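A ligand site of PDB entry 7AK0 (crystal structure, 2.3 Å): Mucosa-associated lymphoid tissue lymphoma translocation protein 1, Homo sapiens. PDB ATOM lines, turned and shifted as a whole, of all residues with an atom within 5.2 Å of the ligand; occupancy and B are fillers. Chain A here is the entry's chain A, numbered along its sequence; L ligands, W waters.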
ATOM      1  N   VAL A  20     -18.111 -12.952 -31.256  1.00  0.00           N
ATOM      2  CA  VAL A  20     -18.385 -12.383 -29.943  1.00  0.00           C
ATOM      3  C   VAL A  20     -17.069 -12.152 -29.219  1.00  0.00           C
ATOM      4  O   VAL A  20     -16.101 -12.901 -29.434  1.00  0.00           O
ATOM      5  CB  VAL A  20     -19.342 -13.311 -29.143  1.00  0.00           C
ATOM      6  CG1 VAL A  20     -20.736 -13.368 -29.780  1.00  0.00           C
ATOM      7  CG2 VAL A  20     -18.769 -14.705 -29.003  1.00  0.00           C
ATOM      8  N   ALA A  21     -17.016 -11.123 -28.376  1.00  0.00           N
ATOM      9  CA  ALA A  21     -15.781 -10.838 -27.655  1.00  0.00           C
ATOM     10  C   ALA A  21     -16.025 -10.232 -26.317  1.00  0.00           C
ATOM     11  O   ALA A  21     -16.936  -9.406 -26.186  1.00  0.00           O
ATOM     12  CB  ALA A  21     -14.883  -9.914 -28.480  1.00  0.00           C
ATOM     13  N   LEU A  22     -15.223 -10.624 -25.331  1.00  0.00           N
ATOM     14  CA  LEU A  22     -15.281 -10.086 -23.974  1.00  0.00           C
ATOM     15  C   LEU A  22     -13.882  -9.547 -23.677  1.00  0.00           C
ATOM     16  O   LEU A  22     -12.880 -10.254 -23.859  1.00  0.00           O
ATOM     17  CB  LEU A  22     -15.690 -11.144 -22.935  1.00  0.00           C
ATOM     18  CG  LEU A  22     -15.509 -10.727 -21.443  1.00  0.00           C
ATOM     19  CD1 LEU A  22     -16.442  -9.525 -21.073  1.00  0.00           C
ATOM     20  CD2 LEU A  22     -15.765 -11.907 -20.519  1.00  0.00           C
ATOM     21  N   LYS A  55     -19.436  -8.701 -31.799  1.00  0.00           N
ATOM     22  CA  LYS A  55     -20.362  -8.155 -30.792  1.00  0.00           C
ATOM     23  C   LYS A  55     -19.451  -8.092 -29.555  1.00  0.00           C
ATOM     24  O   LYS A  55     -18.982  -9.138 -29.103  1.00  0.00           O
ATOM     25  CB  LYS A  55     -21.485  -9.167 -30.529  1.00  0.00           C
ATOM     26  CG  LYS A  55     -22.552  -9.225 -31.621  1.00  0.00           C
ATOM     27  CD  LYS A  55     -23.507 -10.361 -31.401  1.00  0.00           C
ATOM     28  CE  LYS A  55     -24.282 -10.656 -32.650  1.00  0.00           C
ATOM     29  NZ  LYS A  55     -25.182 -11.803 -32.462  1.00  0.00           N
ATOM     30  N   VAL A  56     -19.103  -6.901 -29.064  1.00  0.00           N
ATOM     31  CA  VAL A  56     -18.112  -6.774 -27.987  1.00  0.00           C
ATOM     32  C   VAL A  56     -18.710  -6.298 -26.680  1.00  0.00           C
ATOM     33  O   VAL A  56     -19.509  -5.374 -26.670  1.00  0.00           O
ATOM     34  CB  VAL A  56     -16.965  -5.795 -28.422  1.00  0.00           C
ATOM     35  CG1 VAL A  56     -15.838  -5.771 -27.407  1.00  0.00           C
ATOM     36  CG2 VAL A  56     -16.435  -6.131 -29.819  1.00  0.00           C
ATOM     37  N   VAL A  57     -18.273  -6.881 -25.573  1.00  0.00           N
ATOM     38  CA  VAL A  57     -18.619  -6.397 -24.242  1.00  0.00           C
ATOM     39  C   VAL A  57     -17.259  -6.076 -23.588  1.00  0.00           C
ATOM     40  O   VAL A  57     -16.362  -6.924 -23.601  1.00  0.00           O
ATOM     41  CB  VAL A  57     -19.495  -7.349 -23.415  1.00  0.00           C
ATOM     42  CG1 VAL A  57     -19.467  -6.966 -21.931  1.00  0.00           C
ATOM     43  CG2 VAL A  57     -20.935  -7.355 -23.929  1.00  0.00           C
ATOM     44  N   LEU A  59     -15.392  -4.556 -20.195  1.00  0.00           N
ATOM     45  CA  LEU A  59     -15.554  -4.276 -18.790  1.00  0.00           C
ATOM     46  C   LEU A  59     -14.260  -3.852 -18.137  1.00  0.00           C
ATOM     47  O   LEU A  59     -13.204  -4.424 -18.395  1.00  0.00           O
ATOM     48  CB  LEU A  59     -16.116  -5.531 -18.096  1.00  0.00           C
ATOM     49  CG  LEU A  59     -17.480  -5.996 -18.623  1.00  0.00           C
ATOM     50  CD1 LEU A  59     -17.797  -7.428 -18.170  1.00  0.00           C
ATOM     51  CD2 LEU A  59     -18.585  -5.061 -18.153  1.00  0.00           C
ATOM     52  N   LEU A  62     -12.833  -5.315 -12.635  1.00  0.00           N
ATOM     53  CA  LEU A  62     -13.711  -6.368 -12.112  1.00  0.00           C
ATOM     54  C   LEU A  62     -13.126  -7.081 -10.910  1.00  0.00           C
ATOM     55  O   LEU A  62     -11.919  -7.364 -10.888  1.00  0.00           O
ATOM     56  CB  LEU A  62     -14.068  -7.380 -13.215  1.00  0.00           C
ATOM     57  CG  LEU A  62     -14.815  -6.841 -14.446  1.00  0.00           C
ATOM     58  CD1 LEU A  62     -15.214  -8.004 -15.391  1.00  0.00           C
ATOM     59  CD2 LEU A  62     -16.077  -6.061 -14.047  1.00  0.00           C
ATOM     60  N   THR A  63     -13.979  -7.387  -9.911  1.00  0.00           N
ATOM     61  CA  THR A  63     -13.616  -8.172  -8.756  1.00  0.00           C
ATOM     62  C   THR A  63     -13.575  -9.657  -9.194  1.00  0.00           C
ATOM     63  O   THR A  63     -13.850  -9.995 -10.357  1.00  0.00           O
ATOM     64  CB  THR A  63     -14.617  -7.931  -7.585  1.00  0.00           C
ATOM     65  OG1 THR A  63     -15.877  -8.446  -7.992  1.00  0.00           O
ATOM     66  CG2 THR A  63     -14.738  -6.437  -7.178  1.00  0.00           C
ATOM     67  N   TYR A  65     -15.485 -12.369  -8.375  1.00  0.00           N
ATOM     68  CA  TYR A  65     -16.773 -12.902  -8.764  1.00  0.00           C
ATOM     69  C   TYR A  65     -17.288 -12.269 -10.050  1.00  0.00           C
ATOM     70  O   TYR A  65     -17.853 -12.965 -10.884  1.00  0.00           O
ATOM     71  CB  TYR A  65     -17.762 -12.826  -7.587  1.00  0.00           C
ATOM     72  CG  TYR A  65     -17.553 -13.859  -6.490  1.00  0.00           C
ATOM     73  CD1 TYR A  65     -16.401 -14.631  -6.440  1.00  0.00           C
ATOM     74  CD2 TYR A  65     -18.524 -14.109  -5.538  1.00  0.00           C
ATOM     75  CE1 TYR A  65     -16.198 -15.589  -5.464  1.00  0.00           C
ATOM     76  CE2 TYR A  65     -18.352 -15.082  -4.558  1.00  0.00           C
ATOM     77  CZ  TYR A  65     -17.179 -15.823  -4.528  1.00  0.00           C
ATOM     78  OH  TYR A  65     -16.972 -16.811  -3.592  1.00  0.00           O
ATOM     79  N   GLU A  66     -17.035 -10.979 -10.253  1.00  0.00           N
ATOM     80  CA  GLU A  66     -17.443 -10.300 -11.478  1.00  0.00           C
ATOM     81  C   GLU A  66     -16.736 -10.916 -12.683  1.00  0.00           C
ATOM     82  O   GLU A  66     -17.409 -11.333 -13.620  1.00  0.00           O
ATOM     83  CB  GLU A  66     -17.179  -8.783 -11.376  1.00  0.00           C
ATOM     84  CG  GLU A  66     -18.087  -8.119 -10.357  1.00  0.00           C
ATOM     85  CD  GLU A  66     -17.720  -6.699  -9.945  1.00  0.00           C
ATOM     86  OE1 GLU A  66     -16.657  -6.197 -10.381  1.00  0.00           O
ATOM     87  OE2 GLU A  66     -18.511  -6.084  -9.208  1.00  0.00           O
ATOM     88  N   ASN A  69     -18.087 -14.547 -13.316  1.00  0.00           N
ATOM     89  CA  ASN A  69     -19.416 -14.481 -13.921  1.00  0.00           C
ATOM     90  C   ASN A  69     -19.380 -14.021 -15.364  1.00  0.00           C
ATOM     91  O   ASN A  69     -20.068 -14.624 -16.181  1.00  0.00           O
ATOM     92  CB  ASN A  69     -20.331 -13.601 -13.092  1.00  0.00           C
ATOM     93  CG  ASN A  69     -20.713 -14.241 -11.777  1.00  0.00           C
ATOM     94  OD1 ASN A  69     -20.655 -15.465 -11.625  1.00  0.00           O
ATOM     95  ND2 ASN A  69     -21.126 -13.426 -10.824  1.00  0.00           N
ATOM     96  N   ALA A  70     -18.595 -12.956 -15.681  1.00  0.00           N
ATOM     97  CA  ALA A  70     -18.443 -12.450 -17.042  1.00  0.00           C
ATOM     98  C   ALA A  70     -17.836 -13.517 -17.981  1.00  0.00           C
ATOM     99  O   ALA A  70     -18.334 -13.701 -19.095  1.00  0.00           O
ATOM    100  CB  ALA A  70     -17.572 -11.203 -17.039  1.00  0.00           C
ATOM    101  N   GLU A  73     -20.373 -16.331 -18.598  1.00  0.00           N
ATOM    102  CA  GLU A  73     -21.431 -15.918 -19.502  1.00  0.00           C
ATOM    103  C   GLU A  73     -20.943 -15.751 -20.921  1.00  0.00           C
ATOM    104  O   GLU A  73     -21.702 -16.048 -21.843  1.00  0.00           O
ATOM    105  CB  GLU A  73     -22.157 -14.656 -18.986  1.00  0.00           C
ATOM    106  CG  GLU A  73     -23.177 -15.000 -17.904  1.00  0.00           C
ATOM    107  CD  GLU A  73     -24.074 -13.873 -17.434  1.00  0.00           C
ATOM    108  OE1 GLU A  73     -24.252 -12.875 -18.180  1.00  0.00           O
ATOM    109  OE2 GLU A  73     -24.578 -13.979 -16.295  1.00  0.00           O
ATOM    110  N   PHE A  74     -19.673 -15.348 -21.117  1.00  0.00           N
ATOM    111  CA  PHE A  74     -19.068 -15.277 -22.440  1.00  0.00           C
ATOM    112  C   PHE A  74     -18.962 -16.701 -23.013  1.00  0.00           C
ATOM    113  O   PHE A  74     -19.249 -16.917 -24.187  1.00  0.00           O
ATOM    114  CB  PHE A  74     -17.698 -14.599 -22.408  1.00  0.00           C
ATOM    115  CG  PHE A  74     -16.780 -14.907 -23.577  1.00  0.00           C
ATOM    116  CD1 PHE A  74     -16.900 -14.223 -24.772  1.00  0.00           C
ATOM    117  CD2 PHE A  74     -15.774 -15.865 -23.465  1.00  0.00           C
ATOM    118  CE1 PHE A  74     -16.045 -14.500 -25.834  1.00  0.00           C
ATOM    119  CE2 PHE A  74     -14.964 -16.171 -24.546  1.00  0.00           C
ATOM    120  CZ  PHE A  74     -15.086 -15.465 -25.713  1.00  0.00           C
ATOM    121  N   LEU A  77     -21.946 -18.299 -24.914  1.00  0.00           N
ATOM    122  CA  LEU A  77     -22.226 -17.824 -26.269  1.00  0.00           C
ATOM    123  C   LEU A  77     -21.515 -18.639 -27.347  1.00  0.00           C
ATOM    124  O   LEU A  77     -21.809 -18.482 -28.519  1.00  0.00           O
ATOM    125  CB  LEU A  77     -21.732 -16.377 -26.407  1.00  0.00           C
ATOM    126  CG  LEU A  77     -22.255 -15.368 -25.383  1.00  0.00           C
ATOM    127  CD1 LEU A  77     -21.285 -14.235 -25.247  1.00  0.00           C
ATOM    128  CD2 LEU A  77     -23.595 -14.838 -25.781  1.00  0.00           C
ATOM    129  N   ARG A 252     -27.692 -14.510 -28.626  1.00  0.00           N
ATOM    130  CA  ARG A 252     -26.456 -13.732 -28.707  1.00  0.00           C
ATOM    131  C   ARG A 252     -26.731 -12.288 -29.042  1.00  0.00           C
ATOM    132  O   ARG A 252     -26.163 -11.397 -28.405  1.00  0.00           O
ATOM    133  CB  ARG A 252     -25.469 -14.320 -29.718  1.00  0.00           C
ATOM    134  CG  ARG A 252     -24.856 -15.622 -29.256  1.00  0.00           C
ATOM    135  CD  ARG A 252     -23.768 -16.102 -30.210  1.00  0.00           C
ATOM    136  NE  ARG A 252     -24.329 -16.373 -31.527  1.00  0.00           N
ATOM    137  CZ  ARG A 252     -24.656 -17.582 -31.968  1.00  0.00           C
ATOM    138  NH1 ARG A 252     -25.198 -17.737 -33.176  1.00  0.00           N
ATOM    139  NH2 ARG A 252     -24.476 -18.656 -31.205  1.00  0.00           N
ATOM    140  N   GLN A 255     -28.191 -10.551 -25.856  1.00  0.00           N
ATOM    141  CA  GLN A 255     -27.188 -10.237 -24.816  1.00  0.00           C
ATOM    142  C   GLN A 255     -26.411  -8.984 -25.224  1.00  0.00           C
ATOM    143  O   GLN A 255     -26.256  -8.090 -24.426  1.00  0.00           O
ATOM    144  CB  GLN A 255     -26.217 -11.415 -24.618  1.00  0.00           C
ATOM    145  CG  GLN A 255     -26.873 -12.677 -24.099  1.00  0.00           C
ATOM    146  CD  GLN A 255     -27.038 -12.569 -22.619  1.00  0.00           C
ATOM    147  OE1 GLN A 255     -26.054 -12.641 -21.878  1.00  0.00           O
ATOM    148  NE2 GLN A 255     -28.261 -12.326 -22.159  1.00  0.00           N
ATOM    149  N   TRP A 256     -25.983  -8.900 -26.501  1.00  0.00           N
ATOM    150  CA  TRP A 256     -25.296  -7.723 -27.005  1.00  0.00           C
ATOM    151  C   TRP A 256     -26.172  -6.477 -26.862  1.00  0.00           C
ATOM    152  O   TRP A 256     -25.737  -5.469 -26.297  1.00  0.00           O
ATOM    153  CB  TRP A 256     -24.876  -7.922 -28.474  1.00  0.00           C
ATOM    154  CG  TRP A 256     -24.143  -6.741 -29.025  1.00  0.00           C
ATOM    155  CD1 TRP A 256     -22.815  -6.469 -28.887  1.00  0.00           C
ATOM    156  CD2 TRP A 256     -24.720  -5.592 -29.680  1.00  0.00           C
ATOM    157  NE1 TRP A 256     -22.519  -5.257 -29.467  1.00  0.00           N
ATOM    158  CE2 TRP A 256     -23.675  -4.698 -29.955  1.00  0.00           C
ATOM    159  CE3 TRP A 256     -26.028  -5.233 -30.040  1.00  0.00           C
ATOM    160  CZ2 TRP A 256     -23.897  -3.456 -30.558  1.00  0.00           C
ATOM    161  CZ3 TRP A 256     -26.263  -3.981 -30.600  1.00  0.00           C
ATOM    162  CH2 TRP A 256     -25.194  -3.124 -30.884  1.00  0.00           C
ATOM    163  N   GLN A 352     -21.744  -2.646 -13.165  1.00  0.00           N
ATOM    164  CA  GLN A 352     -21.934  -4.061 -12.838  1.00  0.00           C
ATOM    165  C   GLN A 352     -22.324  -4.280 -11.373  1.00  0.00           C
ATOM    166  O   GLN A 352     -22.743  -5.379 -11.019  1.00  0.00           O
ATOM    167  CB  GLN A 352     -20.698  -4.907 -13.248  1.00  0.00           C
ATOM    168  CG  GLN A 352     -19.565  -4.884 -12.249  1.00  0.00           C
ATOM    169  CD  GLN A 352     -18.705  -3.656 -12.309  1.00  0.00           C
ATOM    170  OE1 GLN A 352     -18.931  -2.720 -13.066  1.00  0.00           O
ATOM    171  NE2 GLN A 352     -17.640  -3.639 -11.542  1.00  0.00           N
ATOM    172  N   LYS A 353     -22.176  -3.268 -10.504  1.00  0.00           N
ATOM    173  CA  LYS A 353     -22.565  -3.375  -9.093  1.00  0.00           C
ATOM    174  C   LYS A 353     -24.015  -2.861  -8.853  1.00  0.00           C
ATOM    175  O   LYS A 353     -24.505  -2.948  -7.735  1.00  0.00           O
ATOM    176  CB  LYS A 353     -21.576  -2.607  -8.216  1.00  0.00           C
ATOM    177  CG  LYS A 353     -20.160  -3.132  -8.346  1.00  0.00           C
ATOM    178  CD  LYS A 353     -19.182  -2.392  -7.458  1.00  0.00           C
ATOM    179  CE  LYS A 353     -17.777  -2.482  -7.997  1.00  0.00           C
ATOM    180  NZ  LYS A 353     -17.285  -3.893  -8.075  1.00  0.00           N
ATOM    181  N   ILE A 388     -24.234  -2.938 -19.035  1.00  0.00           N
ATOM    182  CA  ILE A 388     -24.046  -4.253 -18.420  1.00  0.00           C
ATOM    183  C   ILE A 388     -25.082  -4.564 -17.333  1.00  0.00           C
ATOM    184  O   ILE A 388     -25.479  -5.715 -17.193  1.00  0.00           O
ATOM    185  CB  ILE A 388     -22.609  -4.465 -17.925  1.00  0.00           C
ATOM    186  CG1 ILE A 388     -22.266  -5.967 -17.832  1.00  0.00           C
ATOM    187  CG2 ILE A 388     -22.350  -3.727 -16.607  1.00  0.00           C
ATOM    188  CD1 ILE A 388     -22.290  -6.638 -19.189  1.00  0.00           C
ATOM    189  N   LEU A 391     -28.184  -6.893 -17.941  1.00  0.00           N
ATOM    190  CA  LEU A 391     -28.005  -8.331 -17.867  1.00  0.00           C
ATOM    191  C   LEU A 391     -28.294  -8.920 -16.471  1.00  0.00           C
ATOM    192  O   LEU A 391     -28.166 -10.131 -16.280  1.00  0.00           O
ATOM    193  CB  LEU A 391     -26.588  -8.725 -18.330  1.00  0.00           C
ATOM    194  CG  LEU A 391     -26.231  -8.398 -19.781  1.00  0.00           C
ATOM    195  CD1 LEU A 391     -24.898  -8.977 -20.145  1.00  0.00           C
ATOM    196  CD2 LEU A 391     -27.236  -8.974 -20.747  1.00  0.00           C
ATOM    197  N   ASP A 392     -28.715  -8.076 -15.516  1.00  0.00           N
ATOM    198  CA  ASP A 392     -29.064  -8.472 -14.138  1.00  0.00           C
ATOM    199  C   ASP A 392     -27.853  -8.938 -13.323  1.00  0.00           C
ATOM    200  O   ASP A 392     -27.410 -10.094 -13.382  1.00  0.00           O
ATOM    201  CB  ASP A 392     -30.238  -9.469 -14.091  1.00  0.00           C
ATOM    202  CG  ASP A 392     -31.517  -8.855 -14.662  1.00  0.00           C
ATOM    203  OD1 ASP A 392     -31.704  -7.629 -14.497  1.00  0.00           O
ATOM    204  OD2 ASP A 392     -32.314  -9.609 -15.275  1.00  0.00           O
ATOM    205  N   MET A 393     -27.334  -8.011 -12.552  1.00  0.00           N
ATOM    206  CA  MET A 393     -26.165  -8.160 -11.720  1.00  0.00           C
ATOM    207  C   MET A 393     -26.570  -8.719 -10.356  1.00  0.00           C
ATOM    208  O   MET A 393     -27.640  -8.378  -9.818  1.00  0.00           O
ATOM    209  CB  MET A 393     -25.482  -6.803 -11.612  1.00  0.00           C
ATOM    210  CG  MET A 393     -25.213  -6.197 -12.991  1.00  0.00           C
ATOM    211  SD  MET A 393     -23.874  -7.081 -13.827  1.00  0.00           S
ATOM    212  CE  MET A 393     -24.760  -8.052 -15.061  1.00  0.00           C
ATOM    213  N   HIS A 394     -25.755  -9.620  -9.822  1.00  0.00           N
ATOM    214  CA  HIS A 394     -26.103 -10.310  -8.597  1.00  0.00           C
ATOM    215  C   HIS A 394     -24.924 -10.544  -7.654  1.00  0.00           C
ATOM    216  O   HIS A 394     -23.769 -10.604  -8.078  1.00  0.00           O
ATOM    217  CB  HIS A 394     -26.749 -11.676  -8.941  1.00  0.00           C
ATOM    218  CG  HIS A 394     -25.954 -12.484  -9.933  1.00  0.00           C
ATOM    219  ND1 HIS A 394     -24.843 -13.218  -9.540  1.00  0.00           N
ATOM    220  CD2 HIS A 394     -26.100 -12.604 -11.274  1.00  0.00           C
ATOM    221  CE1 HIS A 394     -24.397 -13.812 -10.647  1.00  0.00           C
ATOM    222  NE2 HIS A 394     -25.115 -13.450 -11.713  1.00  0.00           N
ATOM    223  N   GLY A 396     -22.701 -13.044  -5.480  1.00  0.00           N
ATOM    224  CA  GLY A 396     -22.324 -14.431  -5.613  1.00  0.00           C
ATOM    225  C   GLY A 396     -21.881 -14.919  -6.968  1.00  0.00           C
ATOM    226  O   GLY A 396     -21.862 -14.170  -7.948  1.00  0.00           O
HETATM  227  C1  LIG L   1     -21.745 -10.731 -25.746  1.00  0.00           C
HETATM  228  C2  LIG L   1     -20.349 -10.788 -25.853  1.00  0.00           C
HETATM  229  C3  LIG L   1     -19.591 -10.979 -24.698  1.00  0.00           C
HETATM  230  C4  LIG L   1     -21.492 -10.479 -18.403  1.00  0.00           C
HETATM  231  C5  LIG L   1     -22.743 -11.178 -14.969  1.00  0.00           C
HETATM  232  C6  LIG L   1     -21.968 -10.533 -15.950  1.00  0.00           C
HETATM  233  C7  LIG L   1     -21.012  -9.613 -15.558  1.00  0.00           C
HETATM  234  C8  LIG L   1     -20.831  -9.317 -14.210  1.00  0.00           C
HETATM  235  C9  LIG L   1     -21.589  -9.941 -13.212  1.00  0.00           C
HETATM  236  C10 LIG L   1     -22.555 -10.870 -13.620  1.00  0.00           C
HETATM  237  C11 LIG L   1     -21.099 -10.085  -9.794  1.00  0.00           C
HETATM  238  C12 LIG L   1     -21.566  -8.715  -9.967  1.00  0.00           C
HETATM  239  C13 LIG L   1     -21.744  -8.559 -11.272  1.00  0.00           C
HETATM  240  C14 LIG L   1     -21.745  -7.690  -8.880  1.00  0.00           C
HETATM  241  C15 LIG L   1     -20.223 -11.065 -23.455  1.00  0.00           C
HETATM  242  C16 LIG L   1     -21.615 -10.968 -23.361  1.00  0.00           C
HETATM  243  C17 LIG L   1     -22.367 -10.814 -24.512  1.00  0.00           C
HETATM  244  O1  LIG L   1     -19.442 -11.163 -22.304  1.00  0.00           O
HETATM  245  C18 LIG L   1     -20.071 -11.553 -21.074  1.00  0.00           C
HETATM  246  C19 LIG L   1     -21.349 -10.692 -20.859  1.00  0.00           C
HETATM  247  C20 LIG L   1     -22.321 -11.076 -22.001  1.00  0.00           C
HETATM  248  N1  LIG L   1     -21.943 -10.985 -19.575  1.00  0.00           N
HETATM  249  N2  LIG L   1     -22.168 -10.882 -17.307  1.00  0.00           N
HETATM  250  O2  LIG L   1     -20.560  -9.665 -18.363  1.00  0.00           O
HETATM  251  N3  LIG L   1     -21.428  -9.662 -11.894  1.00  0.00           N
HETATM  252 CL1  LIG L   1     -19.619  -8.124 -13.831  1.00  0.00          CL
HETATM  253  N4  LIG L   1     -21.094 -10.592 -10.958  1.00  0.00           N
HETATM  254  N5  LIG L   1     -20.461  -7.463  -8.171  1.00  0.00           N
HETATM  255 BR1  LIG L   1     -22.813 -10.662 -27.263  1.00  0.00          BR
HETATM  256  O   HOH W   1     -20.081 -10.245  -6.314  1.00  0.00           O
HETATM  257  O   HOH W   2     -21.718  -5.534  -5.683  1.00  0.00           O
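The side-chain carboxylate of Glu 73 lies within hydrogen-bond range of a nitrogen (N2) of the ligand.
The side-chain carboxylate (OE2) of Glu 66 is in salt-bridge range of a nitrogen (N5) of the ligand (2.6 Å).
ND2 of Asn 69 sits at hydrogen-bond distance from N4 of the ligand (2.8 Å).
NE2 of Gln 352 sits close to NZ of Lys 353 (3.5 Å).
The backbone carbonyl oxygen (O) of Gly 396 sits at hydrogen-bond distance from the side-chain amide nitrogen (ND2) of Asn 69 (3.1 Å).
OE2 of Glu 66 is in salt-bridge range of NZ of Lys 353 (2.8 Å).
O of Lys 55 lies within hydrogen-bond range of N of Ala 21, at 2.9 Å.
The backbone carbonyl oxygen (O) of Tyr 65 sits close to the side-chain amide nitrogen (ND2) of Asn 69, 3.3 Å away.
N of Val 57 lies within hydrogen-bond range of O of Ala 21, 2.9 Å away.
NE2 of Gln 352 lies within hydrogen-bond range of OE1 of Glu 66 (3.0 Å).
OE1 of Glu 66 lies within hydrogen-bond range of N of Thr 63.
Residues that only touch the ligand: His 394 (3.2 Å), Gln 352 (3.3 Å), Ala 70 (3.4 Å), Ala 21 (3.4 Å), Leu 59 (3.6 Å), Leu 77 (3.6 Å), Ile 388 (3.6 Å), Arg 252 (3.6 Å), Leu 391 (3.6 Å), Leu 22 (3.6 Å), Trp 256 (3.6 Å), Met 393 (3.6 Å), Val 57 (3.7 Å), Phe 74 (3.8 Å), Lys 55 (3.8 Å) and Gln 255 (3.9 Å).
Hydrophobic or aromatic side chains that line the ligand: Leu 22, Val 57, Leu 59, Ala 70, Phe 74, Leu 77, Trp 256, Ile 388, Leu 391 and Met 393.
Of the 27 residues printed, 19 come within 4 Å of the ligand.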
